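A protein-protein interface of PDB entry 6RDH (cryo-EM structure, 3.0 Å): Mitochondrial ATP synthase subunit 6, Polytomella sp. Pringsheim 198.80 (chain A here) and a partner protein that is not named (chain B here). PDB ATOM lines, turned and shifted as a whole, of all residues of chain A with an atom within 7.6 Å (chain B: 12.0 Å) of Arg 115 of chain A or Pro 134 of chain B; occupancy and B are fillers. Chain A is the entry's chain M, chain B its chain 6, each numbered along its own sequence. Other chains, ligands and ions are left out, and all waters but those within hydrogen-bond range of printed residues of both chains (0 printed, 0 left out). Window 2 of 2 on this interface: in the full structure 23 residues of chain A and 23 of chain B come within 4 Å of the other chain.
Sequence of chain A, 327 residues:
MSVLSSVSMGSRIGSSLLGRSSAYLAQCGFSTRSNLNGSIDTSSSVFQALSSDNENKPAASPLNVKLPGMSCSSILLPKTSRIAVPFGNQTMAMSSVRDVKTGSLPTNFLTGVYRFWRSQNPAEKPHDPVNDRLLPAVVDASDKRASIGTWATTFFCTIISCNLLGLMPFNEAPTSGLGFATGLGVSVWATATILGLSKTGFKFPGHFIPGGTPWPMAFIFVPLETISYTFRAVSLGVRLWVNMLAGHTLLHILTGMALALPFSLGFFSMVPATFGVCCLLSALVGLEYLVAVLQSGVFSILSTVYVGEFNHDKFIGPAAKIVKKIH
Among the printed residues, pairs that only touch across the chains: Asn 108 of chain A with Phe 129 of chain B (3.2 Å), Asn 108 of chain A with Ala 133 of chain B (3.4 Å), Asn 108 of chain A with Thr 136 of chain B (3.4 Å), Arg 115 of chain A with Pro 134 of chain B (3.7 Å), Gly 112 of chain A with Met 132 of chain B (3.8 Å), Asn 108 of chain A with Met 132 of chain B (3.8 Å), Asn 108 of chain A with Arg 130 of chain B (3.8 Å), Phe 109 of chain A with Met 132 of chain B (3.9 Å) and Phe 109 of chain A with Phe 129 of chain B (3.9 Å).
Of chain B, only Pro 134 (3.7 Å) comes within 4 Å of Arg 115 of chain A. Of chain A, only Arg 115 comes within 4 Å of Pro 134 of chain B. Gly 112 of chain A touches one residue of chain B. Val 113 of chain A touches none of the printed residues of chain B. No residue of chain B comes within 4 Å of Tyr 114 of chain A. No residue of chain B comes within 4 Å of Ser 119 of chain A. Of the printed residues of chain A, Ala 133 of chain B touches Asn 108 (3.4 Å). Printed residues of chain B within 4 Å of Phe 109 of chain A: Phe 129 and Met 132. Of the printed residues of chain A, Arg 130 of chain B touches Asn 108 (3.8 Å). Trp 117 of chain A touches none of the printed residues of chain B. Gly 131 of chain B touches none of the printed residues of chain A. The nearest residue of chain A that does not touch Pro 134 of chain B is Thr 111 of chain A (4.1 Å).
Hydrophobic or aromatic side chains of chain A that line the printed part of chain B: Phe 109. Printed residues of chain B that touch a printed residue of chain A: Phe 129, Arg 130, Met 132, Ala 133, Pro 134 and Thr 136. Hydrophobic or aromatic side chains of chain B that line the printed part of chain A: Phe 129, Met 132, Ala 133 and Pro 134.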
ATOM      1  N   ASN A 108      24.022 -11.318 -22.074  1.00  0.00           N
ATOM      2  CA  ASN A 108      23.516  -9.969 -22.311  1.00  0.00           C
ATOM      3  C   ASN A 108      22.924  -9.365 -21.048  1.00  0.00           C
ATOM      4  O   ASN A 108      23.156  -8.189 -20.740  1.00  0.00           O
ATOM      5  CB  ASN A 108      22.467  -9.995 -23.410  1.00  0.00           C
ATOM      6  CG  ASN A 108      23.013 -10.435 -24.719  1.00  0.00           C
ATOM      7  OD1 ASN A 108      22.305 -11.011 -25.535  1.00  0.00           O
ATOM      8  ND2 ASN A 108      24.287 -10.190 -24.934  1.00  0.00           N
ATOM      9  N   PHE A 109      22.173 -10.165 -20.292  1.00  0.00           N
ATOM     10  CA  PHE A 109      21.561  -9.678 -19.065  1.00  0.00           C
ATOM     11  C   PHE A 109      22.605  -9.349 -18.013  1.00  0.00           C
ATOM     12  O   PHE A 109      22.549  -8.283 -17.401  1.00  0.00           O
ATOM     13  CB  PHE A 109      20.578 -10.708 -18.532  1.00  0.00           C
ATOM     14  CG  PHE A 109      19.897 -10.293 -17.273  1.00  0.00           C
ATOM     15  CD1 PHE A 109      19.067  -9.195 -17.256  1.00  0.00           C
ATOM     16  CD2 PHE A 109      20.069 -11.011 -16.110  1.00  0.00           C
ATOM     17  CE1 PHE A 109      18.439  -8.815 -16.106  1.00  0.00           C
ATOM     18  CE2 PHE A 109      19.441 -10.629 -14.958  1.00  0.00           C
ATOM     19  CZ  PHE A 109      18.627  -9.534 -14.957  1.00  0.00           C
ATOM     20  N   LEU A 110      23.580 -10.232 -17.806  1.00  0.00           N
ATOM     21  CA  LEU A 110      24.617  -9.955 -16.824  1.00  0.00           C
ATOM     22  C   LEU A 110      25.546  -8.840 -17.270  1.00  0.00           C
ATOM     23  O   LEU A 110      26.102  -8.144 -16.421  1.00  0.00           O
ATOM     24  CB  LEU A 110      25.423 -11.211 -16.530  1.00  0.00           C
ATOM     25  CG  LEU A 110      25.113 -11.960 -15.243  1.00  0.00           C
ATOM     26  CD1 LEU A 110      25.528 -11.097 -14.084  1.00  0.00           C
ATOM     27  CD2 LEU A 110      23.664 -12.342 -15.134  1.00  0.00           C
ATOM     28  N   THR A 111      25.716  -8.637 -18.577  1.00  0.00           N
ATOM     29  CA  THR A 111      26.468  -7.486 -19.061  1.00  0.00           C
ATOM     30  C   THR A 111      25.761  -6.192 -18.713  1.00  0.00           C
ATOM     31  O   THR A 111      26.382  -5.250 -18.208  1.00  0.00           O
ATOM     32  CB  THR A 111      26.652  -7.583 -20.567  1.00  0.00           C
ATOM     33  OG1 THR A 111      27.199  -8.857 -20.898  1.00  0.00           O
ATOM     34  CG2 THR A 111      27.579  -6.512 -21.047  1.00  0.00           C
ATOM     35  N   GLY A 112      24.452  -6.140 -18.956  1.00  0.00           N
ATOM     36  CA  GLY A 112      23.688  -4.956 -18.606  1.00  0.00           C
ATOM     37  C   GLY A 112      23.637  -4.708 -17.114  1.00  0.00           C
ATOM     38  O   GLY A 112      23.740  -3.566 -16.667  1.00  0.00           O
ATOM     39  N   VAL A 113      23.541  -5.779 -16.325  1.00  0.00           N
ATOM     40  CA  VAL A 113      23.477  -5.648 -14.874  1.00  0.00           C
ATOM     41  C   VAL A 113      24.808  -5.162 -14.317  1.00  0.00           C
ATOM     42  O   VAL A 113      24.847  -4.220 -13.518  1.00  0.00           O
ATOM     43  CB  VAL A 113      23.044  -6.981 -14.243  1.00  0.00           C
ATOM     44  CG1 VAL A 113      23.311  -6.995 -12.779  1.00  0.00           C
ATOM     45  CG2 VAL A 113      21.589  -7.201 -14.466  1.00  0.00           C
ATOM     46  N   TYR A 114      25.917  -5.766 -14.755  1.00  0.00           N
ATOM     47  CA  TYR A 114      27.233  -5.356 -14.281  1.00  0.00           C
ATOM     48  C   TYR A 114      27.562  -3.933 -14.691  1.00  0.00           C
ATOM     49  O   TYR A 114      28.127  -3.178 -13.898  1.00  0.00           O
ATOM     50  CB  TYR A 114      28.311  -6.295 -14.809  1.00  0.00           C
ATOM     51  CG  TYR A 114      29.699  -5.840 -14.445  1.00  0.00           C
ATOM     52  CD1 TYR A 114      30.156  -5.958 -13.154  1.00  0.00           C
ATOM     53  CD2 TYR A 114      30.544  -5.275 -15.389  1.00  0.00           C
ATOM     54  CE1 TYR A 114      31.402  -5.539 -12.807  1.00  0.00           C
ATOM     55  CE2 TYR A 114      31.793  -4.843 -15.041  1.00  0.00           C
ATOM     56  CZ  TYR A 114      32.214  -4.989 -13.747  1.00  0.00           C
ATOM     57  OH  TYR A 114      33.464  -4.577 -13.379  1.00  0.00           O
ATOM     58  N   ARG A 115      27.217  -3.542 -15.916  1.00  0.00           N
ATOM     59  CA  ARG A 115      27.500  -2.179 -16.332  1.00  0.00           C
ATOM     60  C   ARG A 115      26.606  -1.177 -15.623  1.00  0.00           C
ATOM     61  O   ARG A 115      27.040  -0.048 -15.368  1.00  0.00           O
ATOM     62  CB  ARG A 115      27.355  -2.061 -17.837  1.00  0.00           C
ATOM     63  CG  ARG A 115      28.498  -2.687 -18.582  1.00  0.00           C
ATOM     64  CD  ARG A 115      28.219  -2.743 -20.050  1.00  0.00           C
ATOM     65  NE  ARG A 115      27.840  -1.439 -20.556  1.00  0.00           N
ATOM     66  CZ  ARG A 115      28.707  -0.523 -20.954  1.00  0.00           C
ATOM     67  NH1 ARG A 115      28.277   0.641 -21.404  1.00  0.00           N
ATOM     68  NH2 ARG A 115      30.001  -0.771 -20.905  1.00  0.00           N
ATOM     69  N   PHE A 116      25.392  -1.583 -15.236  1.00  0.00           N
ATOM     70  CA  PHE A 116      24.550  -0.720 -14.416  1.00  0.00           C
ATOM     71  C   PHE A 116      25.161  -0.483 -13.049  1.00  0.00           C
ATOM     72  O   PHE A 116      25.234   0.656 -12.585  1.00  0.00           O
ATOM     73  CB  PHE A 116      23.163  -1.319 -14.252  1.00  0.00           C
ATOM     74  CG  PHE A 116      22.216  -0.437 -13.500  1.00  0.00           C
ATOM     75  CD1 PHE A 116      21.595   0.617 -14.129  1.00  0.00           C
ATOM     76  CD2 PHE A 116      21.940  -0.662 -12.170  1.00  0.00           C
ATOM     77  CE1 PHE A 116      20.727   1.420 -13.444  1.00  0.00           C
ATOM     78  CE2 PHE A 116      21.081   0.143 -11.485  1.00  0.00           C
ATOM     79  CZ  PHE A 116      20.472   1.178 -12.120  1.00  0.00           C
ATOM     80  N   TRP A 117      25.592  -1.545 -12.378  1.00  0.00           N
ATOM     81  CA  TRP A 117      26.145  -1.356 -11.044  1.00  0.00           C
ATOM     82  C   TRP A 117      27.535  -0.765 -11.061  1.00  0.00           C
ATOM     83  O   TRP A 117      27.969  -0.216 -10.051  1.00  0.00           O
ATOM     84  CB  TRP A 117      26.161  -2.667 -10.268  1.00  0.00           C
ATOM     85  CG  TRP A 117      24.817  -3.225 -10.058  1.00  0.00           C
ATOM     86  CD1 TRP A 117      24.351  -4.397 -10.527  1.00  0.00           C
ATOM     87  CD2 TRP A 117      23.744  -2.636  -9.325  1.00  0.00           C
ATOM     88  NE1 TRP A 117      23.059  -4.581 -10.151  1.00  0.00           N
ATOM     89  CE2 TRP A 117      22.661  -3.510  -9.407  1.00  0.00           C
ATOM     90  CE3 TRP A 117      23.594  -1.453  -8.608  1.00  0.00           C
ATOM     91  CZ2 TRP A 117      21.453  -3.244  -8.807  1.00  0.00           C
ATOM     92  CZ3 TRP A 117      22.404  -1.191  -8.026  1.00  0.00           C
ATOM     93  CH2 TRP A 117      21.343  -2.075  -8.134  1.00  0.00           C
ATOM     94  N   ARG A 118      28.240  -0.858 -12.177  1.00  0.00           N
ATOM     95  CA  ARG A 118      29.521  -0.190 -12.294  1.00  0.00           C
ATOM     96  C   ARG A 118      29.338   1.291 -12.588  1.00  0.00           C
ATOM     97  O   ARG A 118      30.141   2.110 -12.142  1.00  0.00           O
ATOM     98  CB  ARG A 118      30.352  -0.905 -13.357  1.00  0.00           C
ATOM     99  CG  ARG A 118      31.577  -0.202 -13.859  1.00  0.00           C
ATOM    100  CD  ARG A 118      32.591   0.049 -12.779  1.00  0.00           C
ATOM    101  NE  ARG A 118      33.740   0.784 -13.286  1.00  0.00           N
ATOM    102  CZ  ARG A 118      33.779   2.094 -13.472  1.00  0.00           C
ATOM    103  NH1 ARG A 118      32.734   2.845 -13.198  1.00  0.00           N
ATOM    104  NH2 ARG A 118      34.875   2.658 -13.936  1.00  0.00           N
ATOM    105  N   SER A 119      28.255   1.670 -13.257  1.00  0.00           N
ATOM    106  CA  SER A 119      28.005   3.083 -13.493  1.00  0.00           C
ATOM    107  C   SER A 119      27.526   3.843 -12.264  1.00  0.00           C
ATOM    108  O   SER A 119      27.293   5.046 -12.371  1.00  0.00           O
ATOM    109  CB  SER A 119      26.977   3.236 -14.600  1.00  0.00           C
ATOM    110  OG  SER A 119      25.672   3.098 -14.086  1.00  0.00           O
ATOM    111  N   GLN A 120      27.345   3.189 -11.119  1.00  0.00           N
ATOM    112  CA  GLN A 120      26.863   3.893  -9.937  1.00  0.00           C
ATOM    113  C   GLN A 120      27.971   4.700  -9.286  1.00  0.00           C
ATOM    114  O   GLN A 120      27.729   5.797  -8.778  1.00  0.00           O
ATOM    115  CB  GLN A 120      26.279   2.908  -8.933  1.00  0.00           C
ATOM    116  CG  GLN A 120      25.053   2.211  -9.416  1.00  0.00           C
ATOM    117  CD  GLN A 120      23.986   3.172  -9.815  1.00  0.00           C
ATOM    118  OE1 GLN A 120      23.481   3.129 -10.927  1.00  0.00           O
ATOM    119  NE2 GLN A 120      23.630   4.055  -8.906  1.00  0.00           N
ATOM    120  N   GLY A 149      31.360  -2.299  -8.341  1.00  0.00           N
ATOM    121  CA  GLY A 149      30.577  -2.862  -9.425  1.00  0.00           C
ATOM    122  C   GLY A 149      30.387  -4.352  -9.264  1.00  0.00           C
ATOM    123  O   GLY A 149      29.263  -4.847  -9.304  1.00  0.00           O
ATOM    124  N   THR A 153      26.851  -6.152  -8.037  1.00  0.00           N
ATOM    125  CA  THR A 153      26.122  -7.151  -8.806  1.00  0.00           C
ATOM    126  C   THR A 153      26.149  -8.518  -8.150  1.00  0.00           C
ATOM    127  O   THR A 153      25.218  -9.292  -8.368  1.00  0.00           O
ATOM    128  CB  THR A 153      26.611  -7.243 -10.248  1.00  0.00           C
ATOM    129  OG1 THR A 153      25.897  -8.286 -10.908  1.00  0.00           O
ATOM    130  CG2 THR A 153      28.010  -7.571 -10.321  1.00  0.00           C
ATOM    131  N   TYR B 126      13.437 -10.817 -25.171  1.00  0.00           N
ATOM    132  CA  TYR B 126      14.677 -11.266 -25.798  1.00  0.00           C
ATOM    133  C   TYR B 126      15.420 -10.111 -26.451  1.00  0.00           C
ATOM    134  O   TYR B 126      16.611  -9.905 -26.203  1.00  0.00           O
ATOM    135  CB  TYR B 126      14.386 -12.345 -26.831  1.00  0.00           C
ATOM    136  CG  TYR B 126      15.624 -12.842 -27.516  1.00  0.00           C
ATOM    137  CD1 TYR B 126      16.497 -13.682 -26.863  1.00  0.00           C
ATOM    138  CD2 TYR B 126      15.926 -12.467 -28.809  1.00  0.00           C
ATOM    139  CE1 TYR B 126      17.634 -14.132 -27.470  1.00  0.00           C
ATOM    140  CE2 TYR B 126      17.066 -12.908 -29.421  1.00  0.00           C
ATOM    141  CZ  TYR B 126      17.910 -13.742 -28.747  1.00  0.00           C
ATOM    142  OH  TYR B 126      19.049 -14.188 -29.358  1.00  0.00           O
ATOM    143  N   PHE B 127      14.731  -9.326 -27.266  1.00  0.00           N
ATOM    144  CA  PHE B 127      15.395  -8.211 -27.921  1.00  0.00           C
ATOM    145  C   PHE B 127      15.609  -7.020 -27.007  1.00  0.00           C
ATOM    146  O   PHE B 127      16.276  -6.068 -27.414  1.00  0.00           O
ATOM    147  CB  PHE B 127      14.608  -7.782 -29.147  1.00  0.00           C
ATOM    148  CG  PHE B 127      14.813  -8.668 -30.318  1.00  0.00           C
ATOM    149  CD1 PHE B 127      15.896  -8.494 -31.142  1.00  0.00           C
ATOM    150  CD2 PHE B 127      13.935  -9.691 -30.581  1.00  0.00           C
ATOM    151  CE1 PHE B 127      16.086  -9.315 -32.208  1.00  0.00           C
ATOM    152  CE2 PHE B 127      14.127 -10.516 -31.648  1.00  0.00           C
ATOM    153  CZ  PHE B 127      15.199 -10.327 -32.460  1.00  0.00           C
ATOM    154  N   ALA B 128      15.061  -7.034 -25.798  1.00  0.00           N
ATOM    155  CA  ALA B 128      15.356  -5.987 -24.836  1.00  0.00           C
ATOM    156  C   ALA B 128      16.527  -6.347 -23.949  1.00  0.00           C
ATOM    157  O   ALA B 128      17.266  -5.460 -23.525  1.00  0.00           O
ATOM    158  CB  ALA B 128      14.129  -5.698 -23.975  1.00  0.00           C
ATOM    159  N   PHE B 129      16.699  -7.627 -23.634  1.00  0.00           N
ATOM    160  CA  PHE B 129      17.924  -8.064 -22.979  1.00  0.00           C
ATOM    161  C   PHE B 129      19.091  -7.987 -23.937  1.00  0.00           C
ATOM    162  O   PHE B 129      20.215  -7.693 -23.531  1.00  0.00           O
ATOM    163  CB  PHE B 129      17.783  -9.488 -22.464  1.00  0.00           C
ATOM    164  CG  PHE B 129      16.936  -9.613 -21.243  1.00  0.00           C
ATOM    165  CD1 PHE B 129      16.610  -8.511 -20.485  1.00  0.00           C
ATOM    166  CD2 PHE B 129      16.476 -10.843 -20.850  1.00  0.00           C
ATOM    167  CE1 PHE B 129      15.837  -8.636 -19.370  1.00  0.00           C
ATOM    168  CE2 PHE B 129      15.703 -10.973 -19.736  1.00  0.00           C
ATOM    169  CZ  PHE B 129      15.384  -9.869 -18.996  1.00  0.00           C
ATOM    170  N   ARG B 130      18.834  -8.238 -25.218  1.00  0.00           N
ATOM    171  CA  ARG B 130      19.863  -8.136 -26.243  1.00  0.00           C
ATOM    172  C   ARG B 130      20.346  -6.701 -26.412  1.00  0.00           C
ATOM    173  O   ARG B 130      21.510  -6.475 -26.740  1.00  0.00           O
ATOM    174  CB  ARG B 130      19.298  -8.728 -27.535  1.00  0.00           C
ATOM    175  CG  ARG B 130      19.899  -8.293 -28.820  1.00  0.00           C
ATOM    176  CD  ARG B 130      19.457  -9.209 -29.917  1.00  0.00           C
ATOM    177  NE  ARG B 130      20.178 -10.460 -29.857  1.00  0.00           N
ATOM    178  CZ  ARG B 130      21.259 -10.718 -30.573  1.00  0.00           C
ATOM    179  NH1 ARG B 130      21.726  -9.821 -31.418  1.00  0.00           N
ATOM    180  NH2 ARG B 130      21.856 -11.882 -30.453  1.00  0.00           N
ATOM    181  N   GLY B 131      19.497  -5.719 -26.122  1.00  0.00           N
ATOM    182  CA  GLY B 131      19.931  -4.337 -26.155  1.00  0.00           C
ATOM    183  C   GLY B 131      20.654  -3.859 -24.915  1.00  0.00           C
ATOM    184  O   GLY B 131      21.245  -2.778 -24.944  1.00  0.00           O
ATOM    185  N   MET B 132      20.613  -4.628 -23.824  1.00  0.00           N
ATOM    186  CA  MET B 132      21.348  -4.255 -22.619  1.00  0.00           C
ATOM    187  C   MET B 132      22.844  -4.369 -22.833  1.00  0.00           C
ATOM    188  O   MET B 132      23.615  -3.555 -22.319  1.00  0.00           O
ATOM    189  CB  MET B 132      20.954  -5.142 -21.445  1.00  0.00           C
ATOM    190  CG  MET B 132      19.522  -5.105 -21.060  1.00  0.00           C
ATOM    191  SD  MET B 132      19.208  -6.202 -19.685  1.00  0.00           S
ATOM    192  CE  MET B 132      19.924  -5.263 -18.357  1.00  0.00           C
ATOM    193  N   ALA B 133      23.270  -5.377 -23.550  1.00  0.00           N
ATOM    194  CA  ALA B 133      24.678  -5.537 -23.839  1.00  0.00           C
ATOM    195  C   ALA B 133      25.052  -4.663 -25.018  1.00  0.00           C
ATOM    196  O   ALA B 133      24.355  -4.682 -26.029  1.00  0.00           O
ATOM    197  CB  ALA B 133      24.995  -6.978 -24.165  1.00  0.00           C
ATOM    198  N   PRO B 134      26.137  -3.896 -24.936  1.00  0.00           N
ATOM    199  CA  PRO B 134      26.586  -3.153 -26.114  1.00  0.00           C
ATOM    200  C   PRO B 134      27.154  -4.043 -27.195  1.00  0.00           C
ATOM    201  O   PRO B 134      27.256  -3.599 -28.340  1.00  0.00           O
ATOM    202  CB  PRO B 134      27.654  -2.217 -25.548  1.00  0.00           C
ATOM    203  CG  PRO B 134      27.437  -2.215 -24.107  1.00  0.00           C
ATOM    204  CD  PRO B 134      26.935  -3.552 -23.757  1.00  0.00           C
ATOM    205  N   ALA B 135      27.519  -5.282 -26.865  1.00  0.00           N
ATOM    206  CA  ALA B 135      28.023  -6.222 -27.853  1.00  0.00           C
ATOM    207  C   ALA B 135      26.949  -6.659 -28.829  1.00  0.00           C
ATOM    208  O   ALA B 135      27.258  -6.996 -29.974  1.00  0.00           O
ATOM    209  CB  ALA B 135      28.597  -7.443 -27.154  1.00  0.00           C
ATOM    210  N   THR B 136      25.695  -6.684 -28.405  1.00  0.00           N
ATOM    211  CA  THR B 136      24.611  -7.151 -29.247  1.00  0.00           C
ATOM    212  C   THR B 136      23.618  -6.057 -29.586  1.00  0.00           C
ATOM    213  O   THR B 136      22.676  -6.309 -30.339  1.00  0.00           O
ATOM    214  CB  THR B 136      23.875  -8.307 -28.577  1.00  0.00           C
ATOM    215  OG1 THR B 136      23.276  -7.833 -27.378  1.00  0.00           O
ATOM    216  CG2 THR B 136      24.827  -9.406 -28.224  1.00  0.00           C
ATOM    217  N   ALA B 137      23.800  -4.849 -29.064  1.00  0.00           N
ATOM    218  CA  ALA B 137      22.921  -3.747 -29.409  1.00  0.00           C
ATOM    219  C   ALA B 137      23.184  -3.209 -30.806  1.00  0.00           C
ATOM    220  O   ALA B 137      22.349  -2.471 -31.336  1.00  0.00           O
ATOM    221  CB  ALA B 137      23.072  -2.628 -28.391  1.00  0.00           C
ATOM    222  N   SER B 138      24.317  -3.556 -31.410  1.00  0.00           N
ATOM    223  CA  SER B 138      24.668  -3.101 -32.748  1.00  0.00           C
ATOM    224  C   SER B 138      25.675  -4.081 -33.329  1.00  0.00           C
ATOM    225  O   SER B 138      26.244  -4.906 -32.618  1.00  0.00           O
ATOM    226  CB  SER B 138      25.234  -1.686 -32.715  1.00  0.00           C
ATOM    227  OG  SER B 138      26.452  -1.660 -32.002  1.00  0.00           O
ATOM    228  N   THR B 139      25.889  -3.982 -34.637  1.00  0.00           N
ATOM    229  CA  THR B 139      26.795  -4.893 -35.315  1.00  0.00           C
ATOM    230  C   THR B 139      28.245  -4.466 -35.112  1.00  0.00           C
ATOM    231  O   THR B 139      28.536  -3.408 -34.552  1.00  0.00           O
ATOM    232  CB  THR B 139      26.476  -4.956 -36.803  1.00  0.00           C
ATOM    233  OG1 THR B 139      26.173  -3.640 -37.275  1.00  0.00           O
ATOM    234  CG2 THR B 139      25.295  -5.866 -37.057  1.00  0.00           C
ATOM    235  N   LEU B 140      29.161  -5.302 -35.588  1.00  0.00           N
ATOM    236  CA  LEU B 140      30.580  -5.007 -35.488  1.00  0.00           C
ATOM    237  C   LEU B 140      30.961  -3.876 -36.440  1.00  0.00           C
ATOM    238  O   LEU B 140      30.183  -3.466 -37.303  1.00  0.00           O
ATOM    239  CB  LEU B 140      31.400  -6.249 -35.794  1.00  0.00           C
ATOM    240  CG  LEU B 140      31.836  -7.094 -34.619  1.00  0.00           C
ATOM    241  CD1 LEU B 140      32.785  -8.089 -35.125  1.00  0.00           C
ATOM    242  CD2 LEU B 140      32.514  -6.246 -33.607  1.00  0.00           C
ATOM    243  N   ASN B 141      32.185  -3.373 -36.296  1.00  0.00           N
ATOM    244  CA  ASN B 141      32.490  -2.141 -36.999  1.00  0.00           C
ATOM    245  C   ASN B 141      33.805  -2.086 -37.762  1.00  0.00           C
ATOM    246  O   ASN B 141      33.914  -1.238 -38.649  1.00  0.00           O
ATOM    247  CB  ASN B 141      32.456  -0.970 -36.023  1.00  0.00           C
ATOM    248  CG  ASN B 141      31.968   0.291 -36.663  1.00  0.00           C
ATOM    249  OD1 ASN B 141      31.224   0.250 -37.634  1.00  0.00           O
ATOM    250  ND2 ASN B 141      32.385   1.426 -36.129  1.00  0.00           N
ATOM    251  N   GLY B 142      34.793  -2.922 -37.489  1.00  0.00           N
ATOM    252  CA  GLY B 142      36.074  -2.767 -38.150  1.00  0.00           C
ATOM    253  C   GLY B 142      36.074  -3.254 -39.586  1.00  0.00           C
ATOM    254  O   GLY B 142      35.059  -3.692 -40.116  1.00  0.00           O
